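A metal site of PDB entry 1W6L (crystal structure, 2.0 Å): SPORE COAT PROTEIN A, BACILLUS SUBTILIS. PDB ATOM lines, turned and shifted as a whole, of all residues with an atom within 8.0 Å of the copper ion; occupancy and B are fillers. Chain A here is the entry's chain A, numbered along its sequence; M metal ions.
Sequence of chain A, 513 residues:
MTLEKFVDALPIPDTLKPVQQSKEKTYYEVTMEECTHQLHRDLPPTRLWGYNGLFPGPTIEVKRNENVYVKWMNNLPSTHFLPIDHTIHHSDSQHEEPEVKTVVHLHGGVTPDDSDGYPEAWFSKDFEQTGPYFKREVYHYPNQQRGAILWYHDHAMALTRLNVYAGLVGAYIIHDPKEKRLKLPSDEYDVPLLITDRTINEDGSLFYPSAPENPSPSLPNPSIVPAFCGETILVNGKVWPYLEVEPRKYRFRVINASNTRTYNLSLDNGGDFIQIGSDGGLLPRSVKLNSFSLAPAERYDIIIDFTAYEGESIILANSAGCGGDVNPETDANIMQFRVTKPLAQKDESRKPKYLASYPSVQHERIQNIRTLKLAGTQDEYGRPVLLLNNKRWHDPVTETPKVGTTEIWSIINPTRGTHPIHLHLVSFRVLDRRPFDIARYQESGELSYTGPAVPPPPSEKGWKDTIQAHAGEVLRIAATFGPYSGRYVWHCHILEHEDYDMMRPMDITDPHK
The backbone NH (N) of Ile 494 lies close to the side-chain sulfur (SG) of Cys 492 (3.4 Å). N of Cys 492 sits at hydrogen-bond distance from O of Met 502, at 3.1 Å. The backbone carbonyl oxygen (O) of His 419 is in hydrogen-bond range of the backbone NH (N) of Ala 469 (3.0 Å). NE2 of His 419 lies within hydrogen-bond range of OG1 of Thr 415 (3.0 Å). O of His 497 sits at hydrogen-bond distance from N of Met 502 (2.9 Å). A ring nitrogen (ND1) of His 419 sits close to the side-chain sulfur (SD) of Met 502, 3.6 Å away. The backbone NH (N) of Met 502 lies within hydrogen-bond range of the backbone carbonyl oxygen (O) of Leu 386, 3.1 Å away. The backbone carbonyl oxygen of Pro 226 sits at hydrogen-bond distance from a ring nitrogen (NE2) of His 497 (3.0 Å).
Merely in contact with the copper ion: Ile 494 (3.9 Å) and Met 502 (3.3 Å). Within 4 Å of the copper ion: His 419, Cys 492, Ile 494, His 497 and Met 502. The nearest printed residue that does not touch the copper ion is Pro 420 (4.7 Å).
ND1 of His 497 is bound to the copper ion, at 2.0 Å. The copper ion is bound by a ring nitrogen (ND1) of His 419, at 2.0 Å. The copper ion is bound by the side-chain sulfur (SG) of Cys 492, 2.2 Å away. The copper ion has three donor atoms within binding distance.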
ATOM      1  N   PRO A 226     -24.827  18.160  23.798  1.00  0.00           N
ATOM      2  CA  PRO A 226     -25.429  18.234  22.462  1.00  0.00           C
ATOM      3  C   PRO A 226     -24.558  18.865  21.382  1.00  0.00           C
ATOM      4  O   PRO A 226     -24.983  18.865  20.225  1.00  0.00           O
ATOM      5  CB  PRO A 226     -26.686  19.104  22.681  1.00  0.00           C
ATOM      6  CG  PRO A 226     -26.426  19.875  23.899  1.00  0.00           C
ATOM      7  CD  PRO A 226     -25.445  19.107  24.732  1.00  0.00           C
ATOM      8  N   LEU A 374     -36.577  15.901  11.227  1.00  0.00           N
ATOM      9  CA  LEU A 374     -35.483  16.010  12.169  1.00  0.00           C
ATOM     10  C   LEU A 374     -36.116  16.523  13.456  1.00  0.00           C
ATOM     11  O   LEU A 374     -36.622  17.637  13.492  1.00  0.00           O
ATOM     12  CB  LEU A 374     -34.386  16.962  11.666  1.00  0.00           C
ATOM     13  CG  LEU A 374     -33.814  16.622  10.285  1.00  0.00           C
ATOM     14  CD1 LEU A 374     -32.620  17.558   9.929  1.00  0.00           C
ATOM     15  CD2 LEU A 374     -33.403  15.141  10.156  1.00  0.00           C
ATOM     16  N   LEU A 386     -31.773  13.670  20.202  1.00  0.00           N
ATOM     17  CA  LEU A 386     -32.114  14.014  18.843  1.00  0.00           C
ATOM     18  C   LEU A 386     -32.430  12.745  18.058  1.00  0.00           C
ATOM     19  O   LEU A 386     -31.713  11.750  18.144  1.00  0.00           O
ATOM     20  CB  LEU A 386     -30.994  14.822  18.202  1.00  0.00           C
ATOM     21  CG  LEU A 386     -30.881  16.234  18.794  1.00  0.00           C
ATOM     22  CD1 LEU A 386     -29.594  16.879  18.395  1.00  0.00           C
ATOM     23  CD2 LEU A 386     -32.016  17.088  18.306  1.00  0.00           C
ATOM     24  N   LEU A 387     -33.515  12.800  17.278  1.00  0.00           N
ATOM     25  CA  LEU A 387     -34.082  11.633  16.631  1.00  0.00           C
ATOM     26  C   LEU A 387     -34.382  11.922  15.200  1.00  0.00           C
ATOM     27  O   LEU A 387     -34.828  12.997  14.886  1.00  0.00           O
ATOM     28  CB  LEU A 387     -35.387  11.216  17.327  1.00  0.00           C
ATOM     29  CG  LEU A 387     -35.329  10.852  18.793  1.00  0.00           C
ATOM     30  CD1 LEU A 387     -36.705  10.311  19.257  1.00  0.00           C
ATOM     31  CD2 LEU A 387     -34.261   9.819  19.107  1.00  0.00           C
ATOM     32  N   LEU A 388     -34.127  10.962  14.323  1.00  0.00           N
ATOM     33  CA  LEU A 388     -34.568  11.020  12.931  1.00  0.00           C
ATOM     34  C   LEU A 388     -35.963  10.370  12.858  1.00  0.00           C
ATOM     35  O   LEU A 388     -36.135   9.225  13.289  1.00  0.00           O
ATOM     36  CB  LEU A 388     -33.582  10.268  12.040  1.00  0.00           C
ATOM     37  CG  LEU A 388     -32.122  10.739  12.097  1.00  0.00           C
ATOM     38  CD1 LEU A 388     -31.215   9.760  11.384  1.00  0.00           C
ATOM     39  CD2 LEU A 388     -32.004  12.111  11.486  1.00  0.00           C
ATOM     40  N   ASN A 413     -36.728  20.065   8.523  1.00  0.00           N
ATOM     41  CA  ASN A 413     -36.009  20.524   9.721  1.00  0.00           C
ATOM     42  C   ASN A 413     -36.731  21.649  10.440  1.00  0.00           C
ATOM     43  O   ASN A 413     -36.604  22.794  10.039  1.00  0.00           O
ATOM     44  CB  ASN A 413     -34.603  20.992   9.347  1.00  0.00           C
ATOM     45  CG  ASN A 413     -33.756  21.324  10.562  1.00  0.00           C
ATOM     46  OD1 ASN A 413     -34.178  21.120  11.716  1.00  0.00           O
ATOM     47  ND2 ASN A 413     -32.538  21.807  10.318  1.00  0.00           N
ATOM     48  N   THR A 415     -36.071  22.325  13.639  1.00  0.00           N
ATOM     49  CA  THR A 415     -35.250  22.699  14.782  1.00  0.00           C
ATOM     50  C   THR A 415     -34.603  24.049  14.542  1.00  0.00           C
ATOM     51  O   THR A 415     -34.711  24.597  13.449  1.00  0.00           O
ATOM     52  CB  THR A 415     -34.123  21.625  15.052  1.00  0.00           C
ATOM     53  OG1 THR A 415     -33.136  21.639  14.010  1.00  0.00           O
ATOM     54  CG2 THR A 415     -34.706  20.187  15.036  1.00  0.00           C
ATOM     55  N   GLY A 417     -31.363  24.753  14.328  1.00  0.00           N
ATOM     56  CA  GLY A 417     -30.021  24.720  13.740  1.00  0.00           C
ATOM     57  C   GLY A 417     -29.906  23.843  12.501  1.00  0.00           C
ATOM     58  O   GLY A 417     -30.799  23.069  12.168  1.00  0.00           O
ATOM     59  N   THR A 418     -28.800  23.984  11.804  1.00  0.00           N
ATOM     60  CA  THR A 418     -28.457  23.124  10.664  1.00  0.00           C
ATOM     61  C   THR A 418     -28.001  21.732  11.135  1.00  0.00           C
ATOM     62  O   THR A 418     -27.317  21.612  12.143  1.00  0.00           O
ATOM     63  CB  THR A 418     -27.360  23.795   9.861  1.00  0.00           C
ATOM     64  OG1 THR A 418     -27.875  24.992   9.303  1.00  0.00           O
ATOM     65  CG2 THR A 418     -26.967  22.972   8.653  1.00  0.00           C
ATOM     66  N   HIS A 419     -28.392  20.696  10.410  1.00  0.00           N
ATOM     67  CA  HIS A 419     -27.871  19.351  10.630  1.00  0.00           C
ATOM     68  C   HIS A 419     -27.293  18.857   9.324  1.00  0.00           C
ATOM     69  O   HIS A 419     -27.982  18.875   8.291  1.00  0.00           O
ATOM     70  CB  HIS A 419     -28.973  18.417  11.100  1.00  0.00           C
ATOM     71  CG  HIS A 419     -29.610  18.827  12.393  1.00  0.00           C
ATOM     72  ND1 HIS A 419     -29.221  18.314  13.610  1.00  0.00           N
ATOM     73  CD2 HIS A 419     -30.631  19.682  12.657  1.00  0.00           C
ATOM     74  CE1 HIS A 419     -29.976  18.836  14.568  1.00  0.00           C
ATOM     75  NE2 HIS A 419     -30.833  19.679  14.019  1.00  0.00           N
ATOM     76  N   PRO A 420     -26.007  18.463   9.331  1.00  0.00           N
ATOM     77  CA  PRO A 420     -25.381  17.911   8.143  1.00  0.00           C
ATOM     78  C   PRO A 420     -25.735  16.422   8.007  1.00  0.00           C
ATOM     79  O   PRO A 420     -25.146  15.576   8.674  1.00  0.00           O
ATOM     80  CB  PRO A 420     -23.892  18.111   8.412  1.00  0.00           C
ATOM     81  CG  PRO A 420     -23.774  18.010   9.877  1.00  0.00           C
ATOM     82  CD  PRO A 420     -25.053  18.613  10.447  1.00  0.00           C
ATOM     83  N   ILE A 421     -26.737  16.121   7.179  1.00  0.00           N
ATOM     84  CA  ILE A 421     -27.251  14.754   7.016  1.00  0.00           C
ATOM     85  C   ILE A 421     -26.404  13.991   6.063  1.00  0.00           C
ATOM     86  O   ILE A 421     -26.115  14.448   4.963  1.00  0.00           O
ATOM     87  CB  ILE A 421     -28.736  14.777   6.558  1.00  0.00           C
ATOM     88  CG1 ILE A 421     -29.588  15.555   7.568  1.00  0.00           C
ATOM     89  CG2 ILE A 421     -29.227  13.355   6.280  1.00  0.00           C
ATOM     90  CD1 ILE A 421     -29.540  15.053   8.989  1.00  0.00           C
ATOM     91  N   ALA A 469     -28.834  20.630   6.052  1.00  0.00           N
ATOM     92  CA  ALA A 469     -30.273  20.842   6.104  1.00  0.00           C
ATOM     93  C   ALA A 469     -30.518  21.974   7.091  1.00  0.00           C
ATOM     94  O   ALA A 469     -30.506  21.755   8.304  1.00  0.00           O
ATOM     95  CB  ALA A 469     -30.965  19.588   6.591  1.00  0.00           C
ATOM     96  N   HIS A 491     -27.480   9.324   9.048  1.00  0.00           N
ATOM     97  CA  HIS A 491     -27.398  10.075  10.274  1.00  0.00           C
ATOM     98  C   HIS A 491     -26.962  11.509  10.135  1.00  0.00           C
ATOM     99  O   HIS A 491     -26.406  11.916   9.116  1.00  0.00           O
ATOM    100  CB  HIS A 491     -26.431   9.441  11.241  1.00  0.00           C
ATOM    101  CG  HIS A 491     -25.033   9.296  10.727  1.00  0.00           C
ATOM    102  ND1 HIS A 491     -24.027  10.159  11.084  1.00  0.00           N
ATOM    103  CD2 HIS A 491     -24.478   8.390   9.881  1.00  0.00           C
ATOM    104  CE1 HIS A 491     -22.895   9.755  10.522  1.00  0.00           C
ATOM    105  NE2 HIS A 491     -23.138   8.675   9.814  1.00  0.00           N
ATOM    106  N   CYS A 492     -27.202  12.262  11.199  1.00  0.00           N
ATOM    107  CA  CYS A 492     -26.558  13.571  11.321  1.00  0.00           C
ATOM    108  C   CYS A 492     -25.087  13.364  11.639  1.00  0.00           C
ATOM    109  O   CYS A 492     -24.777  12.510  12.474  1.00  0.00           O
ATOM    110  CB  CYS A 492     -27.210  14.374  12.420  1.00  0.00           C
ATOM    111  SG  CYS A 492     -26.449  15.960  12.642  1.00  0.00           S
ATOM    112  N   HIS A 493     -24.204  14.154  11.015  1.00  0.00           N
ATOM    113  CA  HIS A 493     -22.735  14.035  11.183  1.00  0.00           C
ATOM    114  C   HIS A 493     -22.163  15.014  12.214  1.00  0.00           C
ATOM    115  O   HIS A 493     -20.938  15.136  12.361  1.00  0.00           O
ATOM    116  CB  HIS A 493     -21.937  14.118   9.838  1.00  0.00           C
ATOM    117  CG  HIS A 493     -20.718  13.210   9.804  1.00  0.00           C
ATOM    118  ND1 HIS A 493     -19.750  13.248  10.777  1.00  0.00           N
ATOM    119  CD2 HIS A 493     -20.315  12.252   8.925  1.00  0.00           C
ATOM    120  CE1 HIS A 493     -18.815  12.341  10.510  1.00  0.00           C
ATOM    121  NE2 HIS A 493     -19.142  11.722   9.407  1.00  0.00           N
ATOM    122  N   ILE A 494     -23.027  15.716  12.941  1.00  0.00           N
ATOM    123  CA  ILE A 494     -22.626  16.258  14.227  1.00  0.00           C
ATOM    124  C   ILE A 494     -22.543  15.082  15.182  1.00  0.00           C
ATOM    125  O   ILE A 494     -23.579  14.466  15.507  1.00  0.00           O
ATOM    126  CB  ILE A 494     -23.614  17.341  14.715  1.00  0.00           C
ATOM    127  CG1 ILE A 494     -23.509  18.563  13.813  1.00  0.00           C
ATOM    128  CG2 ILE A 494     -23.310  17.752  16.165  1.00  0.00           C
ATOM    129  CD1 ILE A 494     -24.591  19.575  14.028  1.00  0.00           C
ATOM    130  N   LEU A 495     -21.346  14.761  15.648  1.00  0.00           N
ATOM    131  CA  LEU A 495     -21.096  13.507  16.351  1.00  0.00           C
ATOM    132  C   LEU A 495     -21.814  13.427  17.694  1.00  0.00           C
ATOM    133  O   LEU A 495     -22.289  12.364  18.082  1.00  0.00           O
ATOM    134  CB  LEU A 495     -19.592  13.257  16.512  1.00  0.00           C
ATOM    135  CG  LEU A 495     -18.799  13.244  15.180  1.00  0.00           C
ATOM    136  CD1 LEU A 495     -17.355  12.832  15.408  1.00  0.00           C
ATOM    137  CD2 LEU A 495     -19.442  12.341  14.171  1.00  0.00           C
ATOM    138  N   GLU A 496     -21.923  14.561  18.375  1.00  0.00           N
ATOM    139  CA  GLU A 496     -22.705  14.679  19.596  1.00  0.00           C
ATOM    140  C   GLU A 496     -24.226  14.376  19.378  1.00  0.00           C
ATOM    141  O   GLU A 496     -24.925  13.923  20.314  1.00  0.00           O
ATOM    142  CB  GLU A 496     -22.520  16.083  20.168  1.00  0.00           C
ATOM    143  CG  GLU A 496     -21.173  16.300  20.897  1.00  0.00           C
ATOM    144  CD  GLU A 496     -19.945  16.362  19.978  1.00  0.00           C
ATOM    145  OE1 GLU A 496     -20.085  16.708  18.777  1.00  0.00           O
ATOM    146  OE2 GLU A 496     -18.833  16.033  20.452  1.00  0.00           O
ATOM    147  N   HIS A 497     -24.734  14.645  18.185  1.00  0.00           N
ATOM    148  CA  HIS A 497     -26.111  14.276  17.819  1.00  0.00           C
ATOM    149  C   HIS A 497     -26.190  12.814  17.422  1.00  0.00           C
ATOM    150  O   HIS A 497     -27.062  12.093  17.902  1.00  0.00           O
ATOM    151  CB  HIS A 497     -26.579  15.099  16.625  1.00  0.00           C
ATOM    152  CG  HIS A 497     -26.700  16.566  16.900  1.00  0.00           C
ATOM    153  ND1 HIS A 497     -27.313  17.434  16.020  1.00  0.00           N
ATOM    154  CD2 HIS A 497     -26.260  17.305  17.935  1.00  0.00           C
ATOM    155  CE1 HIS A 497     -27.273  18.665  16.542  1.00  0.00           C
ATOM    156  NE2 HIS A 497     -26.643  18.610  17.699  1.00  0.00           N
ATOM    157  N   GLU A 498     -25.287  12.403  16.535  1.00  0.00           N
ATOM    158  CA  GLU A 498     -25.164  11.024  16.097  1.00  0.00           C
ATOM    159  C   GLU A 498     -25.198  10.008  17.247  1.00  0.00           C
ATOM    160  O   GLU A 498     -25.916   9.000  17.157  1.00  0.00           O
ATOM    161  CB  GLU A 498     -23.898  10.862  15.254  1.00  0.00           C
ATOM    162  CG  GLU A 498     -23.556   9.428  14.872  1.00  0.00           C
ATOM    163  CD  GLU A 498     -22.360   9.330  13.948  1.00  0.00           C
ATOM    164  OE1 GLU A 498     -21.986  10.346  13.334  1.00  0.00           O
ATOM    165  OE2 GLU A 498     -21.799   8.209  13.818  1.00  0.00           O
ATOM    166  N   MET A 502     -29.209  10.380  16.871  1.00  0.00           N
ATOM    167  CA  MET A 502     -29.669  10.854  15.565  1.00  0.00           C
ATOM    168  C   MET A 502     -29.058  10.051  14.423  1.00  0.00           C
ATOM    169  O   MET A 502     -28.426  10.592  13.539  1.00  0.00           O
ATOM    170  CB  MET A 502     -29.363  12.339  15.430  1.00  0.00           C
ATOM    171  CG  MET A 502     -30.249  13.080  14.468  1.00  0.00           C
ATOM    172  SD  MET A 502     -30.000  14.905  14.570  1.00  0.00           S
ATOM    173  CE  MET A 502     -31.105  15.466  13.390  1.00  0.00           C
HETATM  174 CU    CU M   1     -27.659  17.136  14.089  1.00  0.00          CU
